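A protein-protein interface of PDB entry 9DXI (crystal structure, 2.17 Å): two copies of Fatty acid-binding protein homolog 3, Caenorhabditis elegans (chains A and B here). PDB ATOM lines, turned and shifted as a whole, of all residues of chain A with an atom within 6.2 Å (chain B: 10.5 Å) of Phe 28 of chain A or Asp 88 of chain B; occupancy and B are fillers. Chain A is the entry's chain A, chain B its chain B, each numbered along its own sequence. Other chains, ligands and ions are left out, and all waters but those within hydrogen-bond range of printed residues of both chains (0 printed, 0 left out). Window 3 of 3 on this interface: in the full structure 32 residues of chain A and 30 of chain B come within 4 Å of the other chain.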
ATOM      1  N   ASN A  24      27.455  29.021  -4.255  1.00  0.00           N
ATOM      2  CA  ASN A  24      27.064  28.630  -5.610  1.00  0.00           C
ATOM      3  C   ASN A  24      26.031  27.510  -5.623  1.00  0.00           C
ATOM      4  O   ASN A  24      25.897  26.797  -6.623  1.00  0.00           O
ATOM      5  CB  ASN A  24      28.287  28.232  -6.444  1.00  0.00           C
ATOM      6  CG  ASN A  24      29.294  29.361  -6.571  1.00  0.00           C
ATOM      7  OD1 ASN A  24      30.425  29.261  -6.096  1.00  0.00           O
ATOM      8  ND2 ASN A  24      28.882  30.447  -7.211  1.00  0.00           N
ATOM      9  N   PHE A  25      25.297  27.348  -4.520  1.00  0.00           N
ATOM     10  CA  PHE A  25      24.295  26.290  -4.431  1.00  0.00           C
ATOM     11  C   PHE A  25      23.057  26.620  -5.256  1.00  0.00           C
ATOM     12  O   PHE A  25      22.360  25.708  -5.716  1.00  0.00           O
ATOM     13  CB  PHE A  25      23.922  26.062  -2.964  1.00  0.00           C
ATOM     14  CG  PHE A  25      23.073  24.842  -2.728  1.00  0.00           C
ATOM     15  CD1 PHE A  25      23.296  23.675  -3.437  1.00  0.00           C
ATOM     16  CD2 PHE A  25      22.071  24.857  -1.774  1.00  0.00           C
ATOM     17  CE1 PHE A  25      22.521  22.552  -3.214  1.00  0.00           C
ATOM     18  CE2 PHE A  25      21.293  23.738  -1.546  1.00  0.00           C
ATOM     19  CZ  PHE A  25      21.519  22.585  -2.266  1.00  0.00           C
ATOM     20  N   ASP A  26      22.776  27.908  -5.463  1.00  0.00           N
ATOM     21  CA  ASP A  26      21.625  28.295  -6.270  1.00  0.00           C
ATOM     22  C   ASP A  26      21.826  27.921  -7.733  1.00  0.00           C
ATOM     23  O   ASP A  26      20.960  27.281  -8.343  1.00  0.00           O
ATOM     24  CB  ASP A  26      21.364  29.793  -6.137  1.00  0.00           C
ATOM     25  CG  ASP A  26      20.237  30.261  -7.035  1.00  0.00           C
ATOM     26  OD1 ASP A  26      19.062  30.080  -6.657  1.00  0.00           O
ATOM     27  OD2 ASP A  26      20.527  30.792  -8.129  1.00  0.00           O
ATOM     28  N   GLU A  27      22.957  28.323  -8.319  1.00  0.00           N
ATOM     29  CA  GLU A  27      23.200  28.024  -9.727  1.00  0.00           C
ATOM     30  C   GLU A  27      23.430  26.539  -9.942  1.00  0.00           C
ATOM     31  O   GLU A  27      23.187  26.030 -11.040  1.00  0.00           O
ATOM     32  CB  GLU A  27      24.400  28.810 -10.252  1.00  0.00           C
ATOM     33  CG  GLU A  27      24.516  30.221  -9.719  1.00  0.00           C
ATOM     34  CD  GLU A  27      25.312  30.284  -8.435  1.00  0.00           C
ATOM     35  OE1 GLU A  27      24.703  30.285  -7.345  1.00  0.00           O
ATOM     36  OE2 GLU A  27      26.559  30.330  -8.525  1.00  0.00           O
ATOM     37  N   PHE A  28      23.916  25.839  -8.914  1.00  0.00           N
ATOM     38  CA  PHE A  28      24.038  24.390  -8.984  1.00  0.00           C
ATOM     39  C   PHE A  28      22.673  23.739  -9.179  1.00  0.00           C
ATOM     40  O   PHE A  28      22.492  22.895 -10.064  1.00  0.00           O
ATOM     41  CB  PHE A  28      24.718  23.873  -7.715  1.00  0.00           C
ATOM     42  CG  PHE A  28      24.896  22.386  -7.679  1.00  0.00           C
ATOM     43  CD1 PHE A  28      25.966  21.790  -8.321  1.00  0.00           C
ATOM     44  CD2 PHE A  28      23.998  21.580  -6.991  1.00  0.00           C
ATOM     45  CE1 PHE A  28      26.140  20.421  -8.284  1.00  0.00           C
ATOM     46  CE2 PHE A  28      24.164  20.207  -6.952  1.00  0.00           C
ATOM     47  CZ  PHE A  28      25.235  19.627  -7.601  1.00  0.00           C
ATOM     48  N   LEU A  29      21.690  24.132  -8.366  1.00  0.00           N
ATOM     49  CA  LEU A  29      20.348  23.580  -8.512  1.00  0.00           C
ATOM     50  C   LEU A  29      19.708  24.026  -9.819  1.00  0.00           C
ATOM     51  O   LEU A  29      19.038  23.233 -10.488  1.00  0.00           O
ATOM     52  CB  LEU A  29      19.482  23.989  -7.325  1.00  0.00           C
ATOM     53  CG  LEU A  29      19.926  23.491  -5.952  1.00  0.00           C
ATOM     54  CD1 LEU A  29      19.268  24.311  -4.860  1.00  0.00           C
ATOM     55  CD2 LEU A  29      19.606  22.014  -5.786  1.00  0.00           C
ATOM     56  N   ALA A  30      19.906  25.293 -10.195  1.00  0.00           N
ATOM     57  CA  ALA A  30      19.368  25.792 -11.458  1.00  0.00           C
ATOM     58  C   ALA A  30      19.924  25.025 -12.649  1.00  0.00           C
ATOM     59  O   ALA A  30      19.214  24.823 -13.641  1.00  0.00           O
ATOM     60  CB  ALA A  30      19.670  27.285 -11.604  1.00  0.00           C
ATOM     61  N   ALA A  31      21.187  24.596 -12.577  1.00  0.00           N
ATOM     62  CA  ALA A  31      21.753  23.794 -13.653  1.00  0.00           C
ATOM     63  C   ALA A  31      21.200  22.374 -13.661  1.00  0.00           C
ATOM     64  O   ALA A  31      21.332  21.676 -14.672  1.00  0.00           O
ATOM     65  CB  ALA A  31      23.278  23.763 -13.543  1.00  0.00           C
ATOM     66  N   LYS A  32      20.588  21.935 -12.562  1.00  0.00           N
ATOM     67  CA  LYS A  32      19.954  20.627 -12.490  1.00  0.00           C
ATOM     68  C   LYS A  32      18.477  20.664 -12.855  1.00  0.00           C
ATOM     69  O   LYS A  32      17.814  19.622 -12.793  1.00  0.00           O
ATOM     70  CB  LYS A  32      20.117  20.032 -11.086  1.00  0.00           C
ATOM     71  CG  LYS A  32      21.437  19.316 -10.867  1.00  0.00           C
ATOM     72  CD  LYS A  32      21.334  18.336  -9.714  1.00  0.00           C
ATOM     73  CE  LYS A  32      21.158  19.057  -8.390  1.00  0.00           C
ATOM     74  NZ  LYS A  32      20.561  18.164  -7.363  1.00  0.00           N
ATOM     75  N   GLY A  33      17.947  21.828 -13.226  1.00  0.00           N
ATOM     76  CA  GLY A  33      16.565  21.949 -13.635  1.00  0.00           C
ATOM     77  C   GLY A  33      15.588  22.297 -12.534  1.00  0.00           C
ATOM     78  O   GLY A  33      14.380  22.357 -12.800  1.00  0.00           O
ATOM     79  N   GLU A 118      27.104  11.044  -9.546  1.00  0.00           N
ATOM     80  CA  GLU A 118      27.219  12.128  -8.581  1.00  0.00           C
ATOM     81  C   GLU A 118      28.338  11.778  -7.616  1.00  0.00           C
ATOM     82  O   GLU A 118      28.361  10.674  -7.065  1.00  0.00           O
ATOM     83  CB  GLU A 118      25.901  12.353  -7.831  1.00  0.00           C
ATOM     84  CG  GLU A 118      24.853  13.100  -8.640  1.00  0.00           C
ATOM     85  CD  GLU A 118      23.451  12.925  -8.091  1.00  0.00           C
ATOM     86  OE1 GLU A 118      23.293  12.232  -7.064  1.00  0.00           O
ATOM     87  OE2 GLU A 118      22.505  13.480  -8.690  1.00  0.00           O
ATOM     88  N   TYR A 120      30.490  13.297  -4.252  1.00  0.00           N
ATOM     89  CA  TYR A 120      30.610  14.263  -3.172  1.00  0.00           C
ATOM     90  C   TYR A 120      32.001  14.148  -2.570  1.00  0.00           C
ATOM     91  O   TYR A 120      32.455  13.040  -2.265  1.00  0.00           O
ATOM     92  CB  TYR A 120      29.545  14.022  -2.100  1.00  0.00           C
ATOM     93  CG  TYR A 120      28.131  13.984  -2.632  1.00  0.00           C
ATOM     94  CD1 TYR A 120      27.586  12.806  -3.130  1.00  0.00           C
ATOM     95  CD2 TYR A 120      27.335  15.123  -2.630  1.00  0.00           C
ATOM     96  CE1 TYR A 120      26.295  12.764  -3.616  1.00  0.00           C
ATOM     97  CE2 TYR A 120      26.039  15.088  -3.114  1.00  0.00           C
ATOM     98  CZ  TYR A 120      25.526  13.907  -3.606  1.00  0.00           C
ATOM     99  OH  TYR A 120      24.240  13.860  -4.088  1.00  0.00           O
ATOM    100  N   MET A 131      31.779  19.992   1.992  1.00  0.00           N
ATOM    101  CA  MET A 131      31.299  19.140   0.915  1.00  0.00           C
ATOM    102  C   MET A 131      31.386  19.899  -0.402  1.00  0.00           C
ATOM    103  O   MET A 131      30.858  21.008  -0.520  1.00  0.00           O
ATOM    104  CB  MET A 131      29.854  18.707   1.176  1.00  0.00           C
ATOM    105  CG  MET A 131      29.323  17.689   0.180  1.00  0.00           C
ATOM    106  SD  MET A 131      27.581  17.306   0.459  1.00  0.00           S
ATOM    107  CE  MET A 131      26.800  18.682  -0.374  1.00  0.00           C
ATOM    108  N   MET A 133      30.694  19.656  -4.608  1.00  0.00           N
ATOM    109  CA  MET A 133      29.954  18.985  -5.664  1.00  0.00           C
ATOM    110  C   MET A 133      30.252  19.661  -6.991  1.00  0.00           C
ATOM    111  O   MET A 133      30.320  20.890  -7.064  1.00  0.00           O
ATOM    112  CB  MET A 133      28.447  19.029  -5.405  1.00  0.00           C
ATOM    113  CG  MET A 133      28.018  18.530  -4.047  1.00  0.00           C
ATOM    114  SD  MET A 133      26.226  18.333  -3.998  1.00  0.00           S
ATOM    115  CE  MET A 133      25.660  19.990  -3.654  1.00  0.00           C
ATOM    116  N   VAL A 134      30.423  18.860  -8.040  1.00  0.00           N
ATOM    117  CA  VAL A 134      30.654  19.365  -9.391  1.00  0.00           C
ATOM    118  C   VAL A 134      29.665  18.680 -10.324  1.00  0.00           C
ATOM    119  O   VAL A 134      29.741  17.460 -10.521  1.00  0.00           O
ATOM    120  CB  VAL A 134      32.098  19.125  -9.864  1.00  0.00           C
ATOM    121  CG1 VAL A 134      32.382  19.920 -11.135  1.00  0.00           C
ATOM    122  CG2 VAL A 134      33.096  19.481  -8.767  1.00  0.00           C
ATOM    123  N   ASN A 135      28.747  19.453 -10.900  1.00  0.00           N
ATOM    124  CA  ASN A 135      27.765  18.898 -11.819  1.00  0.00           C
ATOM    125  C   ASN A 135      27.347  19.966 -12.818  1.00  0.00           C
ATOM    126  O   ASN A 135      27.109  21.117 -12.442  1.00  0.00           O
ATOM    127  CB  ASN A 135      26.539  18.361 -11.071  1.00  0.00           C
ATOM    128  CG  ASN A 135      25.604  17.574 -11.970  1.00  0.00           C
ATOM    129  OD1 ASN A 135      26.047  16.835 -12.852  1.00  0.00           O
ATOM    130  ND2 ASN A 135      24.304  17.732 -11.754  1.00  0.00           N
ATOM    131  N   ASN A 136      27.263  19.569 -14.090  1.00  0.00           N
ATOM    132  CA  ASN A 136      26.872  20.453 -15.188  1.00  0.00           C
ATOM    133  C   ASN A 136      27.771  21.681 -15.278  1.00  0.00           C
ATOM    134  O   ASN A 136      27.340  22.752 -15.710  1.00  0.00           O
ATOM    135  CB  ASN A 136      25.402  20.870 -15.070  1.00  0.00           C
ATOM    136  CG  ASN A 136      24.453  19.687 -15.159  1.00  0.00           C
ATOM    137  OD1 ASN A 136      23.644  19.455 -14.261  1.00  0.00           O
ATOM    138  ND2 ASN A 136      24.556  18.927 -16.244  1.00  0.00           N
ATOM    139  N   ILE A 138      29.138  23.367 -12.789  1.00  0.00           N
ATOM    140  CA  ILE A 138      29.045  24.265 -11.644  1.00  0.00           C
ATOM    141  C   ILE A 138      29.619  23.557 -10.422  1.00  0.00           C
ATOM    142  O   ILE A 138      29.179  22.457 -10.063  1.00  0.00           O
ATOM    143  CB  ILE A 138      27.604  24.731 -11.389  1.00  0.00           C
ATOM    144  CG1 ILE A 138      27.184  25.788 -12.416  1.00  0.00           C
ATOM    145  CG2 ILE A 138      27.489  25.336 -10.001  1.00  0.00           C
ATOM    146  CD1 ILE A 138      26.772  25.240 -13.764  1.00  0.00           C
ATOM    147  N   THR A 139      30.610  24.183  -9.796  1.00  0.00           N
ATOM    148  CA  THR A 139      31.186  23.719  -8.545  1.00  0.00           C
ATOM    149  C   THR A 139      30.503  24.434  -7.392  1.00  0.00           C
ATOM    150  O   THR A 139      30.383  25.662  -7.399  1.00  0.00           O
ATOM    151  CB  THR A 139      32.690  23.987  -8.498  1.00  0.00           C
ATOM    152  OG1 THR A 139      33.329  23.288  -9.569  1.00  0.00           O
ATOM    153  CG2 THR A 139      33.275  23.527  -7.172  1.00  0.00           C
ATOM    154  N   CYS A 140      30.055  23.672  -6.408  1.00  0.00           N
ATOM    155  CA  CYS A 140      29.366  24.207  -5.245  1.00  0.00           C
ATOM    156  C   CYS A 140      29.990  23.620  -3.990  1.00  0.00           C
ATOM    157  O   CYS A 140      30.442  22.472  -3.995  1.00  0.00           O
ATOM    158  CB  CYS A 140      27.866  23.883  -5.314  1.00  0.00           C
ATOM    159  SG  CYS A 140      26.862  24.556  -3.979  1.00  0.00           S
ATOM    160  N   ARG A 142      29.608  23.331   0.447  1.00  0.00           N
ATOM    161  CA  ARG A 142      28.722  23.469   1.591  1.00  0.00           C
ATOM    162  C   ARG A 142      29.516  23.185   2.853  1.00  0.00           C
ATOM    163  O   ARG A 142      30.298  22.233   2.902  1.00  0.00           O
ATOM    164  CB  ARG A 142      27.515  22.524   1.495  1.00  0.00           C
ATOM    165  CG  ARG A 142      26.868  22.481   0.116  1.00  0.00           C
ATOM    166  CD  ARG A 142      25.477  21.883   0.172  1.00  0.00           C
ATOM    167  NE  ARG A 142      24.536  22.825   0.761  1.00  0.00           N
ATOM    168  CZ  ARG A 142      23.242  22.592   0.916  1.00  0.00           C
ATOM    169  NH1 ARG A 142      22.700  21.440   0.564  1.00  0.00           N
ATOM    170  NH2 ARG A 142      22.472  23.543   1.438  1.00  0.00           N
ATOM    171  N   ALA B  84      11.480  16.733   2.416  1.00  0.00           N
ATOM    172  CA  ALA B  84      12.791  16.233   2.794  1.00  0.00           C
ATOM    173  C   ALA B  84      13.740  16.420   1.623  1.00  0.00           C
ATOM    174  O   ALA B  84      13.341  16.283   0.463  1.00  0.00           O
ATOM    175  CB  ALA B  84      12.738  14.758   3.205  1.00  0.00           C
ATOM    176  N   GLU B  85      14.992  16.734   1.932  1.00  0.00           N
ATOM    177  CA  GLU B  85      15.999  17.025   0.926  1.00  0.00           C
ATOM    178  C   GLU B  85      17.049  15.921   0.906  1.00  0.00           C
ATOM    179  O   GLU B  85      17.468  15.429   1.959  1.00  0.00           O
ATOM    180  CB  GLU B  85      16.656  18.384   1.187  1.00  0.00           C
ATOM    181  CG  GLU B  85      15.880  19.578   0.621  1.00  0.00           C
ATOM    182  CD  GLU B  85      14.563  19.849   1.338  1.00  0.00           C
ATOM    183  OE1 GLU B  85      14.423  19.459   2.516  1.00  0.00           O
ATOM    184  OE2 GLU B  85      13.665  20.462   0.718  1.00  0.00           O
ATOM    185  N   GLY B  86      17.457  15.531  -0.297  1.00  0.00           N
ATOM    186  CA  GLY B  86      18.423  14.470  -0.488  1.00  0.00           C
ATOM    187  C   GLY B  86      19.852  14.968  -0.421  1.00  0.00           C
ATOM    188  O   GLY B  86      20.137  16.079   0.035  1.00  0.00           O
ATOM    189  N   LEU B  87      20.765  14.121  -0.898  1.00  0.00           N
ATOM    190  CA  LEU B  87      22.189  14.429  -0.807  1.00  0.00           C
ATOM    191  C   LEU B  87      22.571  15.577  -1.733  1.00  0.00           C
ATOM    192  O   LEU B  87      23.284  16.502  -1.324  1.00  0.00           O
ATOM    193  CB  LEU B  87      23.014  13.179  -1.128  1.00  0.00           C
ATOM    194  CG  LEU B  87      23.309  12.177  -0.006  1.00  0.00           C
ATOM    195  CD1 LEU B  87      22.066  11.831   0.800  1.00  0.00           C
ATOM    196  CD2 LEU B  87      23.926  10.915  -0.590  1.00  0.00           C
ATOM    197  N   ASP B  88      22.101  15.537  -2.979  1.00  0.00           N
ATOM    198  CA  ASP B  88      22.398  16.565  -3.969  1.00  0.00           C
ATOM    199  C   ASP B  88      21.531  17.811  -3.816  1.00  0.00           C
ATOM    200  O   ASP B  88      21.649  18.728  -4.634  1.00  0.00           O
ATOM    201  CB  ASP B  88      22.245  15.991  -5.386  1.00  0.00           C
ATOM    202  CG  ASP B  88      20.833  15.491  -5.678  1.00  0.00           C
ATOM    203  OD1 ASP B  88      20.150  15.008  -4.750  1.00  0.00           O
ATOM    204  OD2 ASP B  88      20.405  15.572  -6.848  1.00  0.00           O
ATOM    205  N   GLY B  89      20.677  17.871  -2.793  1.00  0.00           N
ATOM    206  CA  GLY B  89      19.808  18.997  -2.555  1.00  0.00           C
ATOM    207  C   GLY B  89      18.371  18.798  -2.995  1.00  0.00           C
ATOM    208  O   GLY B  89      17.478  19.457  -2.443  1.00  0.00           O
ATOM    209  N   VAL B  90      18.127  17.912  -3.965  1.00  0.00           N
ATOM    210  CA  VAL B  90      16.800  17.668  -4.527  1.00  0.00           C
ATOM    211  C   VAL B  90      15.802  17.406  -3.407  1.00  0.00           C
ATOM    212  O   VAL B  90      16.160  16.848  -2.369  1.00  0.00           O
ATOM    213  CB  VAL B  90      16.843  16.502  -5.535  1.00  0.00           C
ATOM    214  CG1 VAL B  90      17.014  15.163  -4.817  1.00  0.00           C
ATOM    215  CG2 VAL B  90      15.593  16.493  -6.399  1.00  0.00           C
ATOM    216  N   ALA B  91      14.556  17.826  -3.596  1.00  0.00           N
ATOM    217  CA  ALA B  91      13.560  17.790  -2.537  1.00  0.00           C
ATOM    218  C   ALA B  91      12.377  16.929  -2.950  1.00  0.00           C
ATOM    219  O   ALA B  91      12.000  16.896  -4.125  1.00  0.00           O
ATOM    220  CB  ALA B  91      13.078  19.201  -2.182  1.00  0.00           C
ATOM    221  N   HIS B  92      11.791  16.239  -1.971  1.00  0.00           N
ATOM    222  CA  HIS B  92      10.621  15.401  -2.177  1.00  0.00           C
ATOM    223  C   HIS B  92       9.537  15.802  -1.188  1.00  0.00           C
ATOM    224  O   HIS B  92       9.833  16.182  -0.051  1.00  0.00           O
ATOM    225  CB  HIS B  92      10.952  13.910  -1.997  1.00  0.00           C
ATOM    226  CG  HIS B  92      12.355  13.545  -2.375  1.00  0.00           C
ATOM    227  ND1 HIS B  92      13.433  13.766  -1.541  1.00  0.00           N
ATOM    228  CD2 HIS B  92      12.856  12.960  -3.488  1.00  0.00           C
ATOM    229  CE1 HIS B  92      14.535  13.339  -2.129  1.00  0.00           C
ATOM    230  NE2 HIS B  92      14.214  12.845  -3.311  1.00  0.00           N
ATOM    231  N   ARG B 109       8.653  13.927  -6.476  1.00  0.00           N
ATOM    232  CA  ARG B 109       9.886  14.681  -6.661  1.00  0.00           C
ATOM    233  C   ARG B 109       9.547  16.038  -7.273  1.00  0.00           C
ATOM    234  O   ARG B 109       8.914  16.101  -8.333  1.00  0.00           O
ATOM    235  CB  ARG B 109      10.854  13.905  -7.554  1.00  0.00           C
ATOM    236  CG  ARG B 109      12.312  14.295  -7.397  1.00  0.00           C
ATOM    237  CD  ARG B 109      13.159  13.674  -8.498  1.00  0.00           C
ATOM    238  NE  ARG B 109      14.587  13.825  -8.248  1.00  0.00           N
ATOM    239  CZ  ARG B 109      15.533  13.595  -9.149  1.00  0.00           C
ATOM    240  NH1 ARG B 109      15.237  13.228 -10.385  1.00  0.00           N
ATOM    241  NH2 ARG B 109      16.809  13.745  -8.803  1.00  0.00           N
ATOM    242  N   ASN B 111      11.706  18.513  -8.361  1.00  0.00           N
ATOM    243  CA  ASN B 111      12.555  18.801  -9.551  1.00  0.00           C
ATOM    244  C   ASN B 111      12.014  18.018 -10.752  1.00  0.00           C
ATOM    245  O   ASN B 111      11.940  18.601 -11.857  1.00  0.00           O
ATOM    246  CB  ASN B 111      14.023  18.497  -9.270  1.00  0.00           C
ATOM    247  CG  ASN B 111      14.824  18.301 -10.535  1.00  0.00           C
ATOM    248  OD1 ASN B 111      15.075  19.263 -11.268  1.00  0.00           O
ATOM    249  ND2 ASN B 111      15.234  17.070 -10.805  1.00  0.00           N
ATOM    250  N   ASP B 112      11.640  16.752 -10.542  1.00  0.00           N
ATOM    251  CA  ASP B 112      11.118  15.897 -11.644  1.00  0.00           C
ATOM    252  C   ASP B 112       9.646  16.240 -11.904  1.00  0.00           C
ATOM    253  O   ASP B 112       8.965  16.676 -10.954  1.00  0.00           O
ATOM    254  CB  ASP B 112      11.339  14.428 -11.324  1.00  0.00           C
ATOM    255  CG  ASP B 112      10.978  13.445 -12.426  1.00  0.00           C
ATOM    256  OD1 ASP B 112      11.837  13.197 -13.298  1.00  0.00           O
ATOM    257  OD2 ASP B 112       9.840  12.934 -12.401  1.00  0.00           O
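The side-chain carboxylate of Asp 88 of chain B is in salt-bridge range of the side-chain amino group of Lys 32 of chain A. The side-chain carboxylate of Glu 118 of chain A sits close to the side-chain carboxylate of Asp 88 of chain B, at 3.5 Å. The side-chain amide oxygen (OD1) of Asn 111 of chain B sits close to the backbone carbonyl oxygen (O) of Lys 32 of chain A (3.2 Å). The backbone NH (N) of Asp 88 of chain B is in hydrogen-bond range of the side-chain hydroxyl (OH) of Tyr 120 of chain A, at 2.9 Å.
The backbone NH (N) of Phe 25 of chain A lies close to the side-chain sulfur (SG) of Cys 140 of chain A (3.2 Å).
Phe 25 of chain A touches Gly 89 of chain B (CZ to CA, 3.99 Å). Phe 28 of chain A touches Asp 88 of chain B (CE2 to O, 3.7 Å). C of Gly 33 of chain A touches OD1 of Asn 111 of chain B (3.3 Å). Tyr 120 of chain A touches Leu 87 of chain B.
Phe 28 of chain A touches one residue of chain B. No residue of chain B comes within 4 Å of Leu 29 of chain A. No residue of chain B comes within 4 Å of Ala 30 of chain A. Of the printed residues of chain B, Glu 118 of chain A touches Asp 88 (3.5 Å). Printed residues of chain B within 4 Å of Tyr 120 of chain A: Leu 87 (3.3 Å) and Asp 88 (2.9 Å). No residue of chain B comes within 4 Å of Met 133 of chain A. No residue of chain B comes within 4 Å of Ile 138 of chain A. Glu 85 of chain B touches none of the printed residues of chain A. Of the printed residues of chain A, Leu 87 of chain B touches Tyr 120. Asp 88 of chain B touches just these residues of chain A: Phe 28, Lys 32, Glu 118 and Tyr 120. Printed residues of chain A within 4 Å of Gly 89 of chain B: Phe 25 (3.99 Å). The nearest residue of chain A that does not touch Asp 88 of chain B is Leu 29 of chain A (4.04 Å). The nearest printed residue of chain B that does not touch Gly 33 of chain A is Asp 112 of chain B (6.6 Å).
Among the printed residues, 8 pairs touch across the chains. Among the printed residues, Asp or Glu carboxylates within 4 Å of a Lys or Arg side-chain nitrogen of the other chain: Lys 32 of chain A with Asp 88 of chain B.
No position is printed for both chains. Of the 8 pairs that touch across the chains among the printed residues, none has its exchanged pair printed and touching as well.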
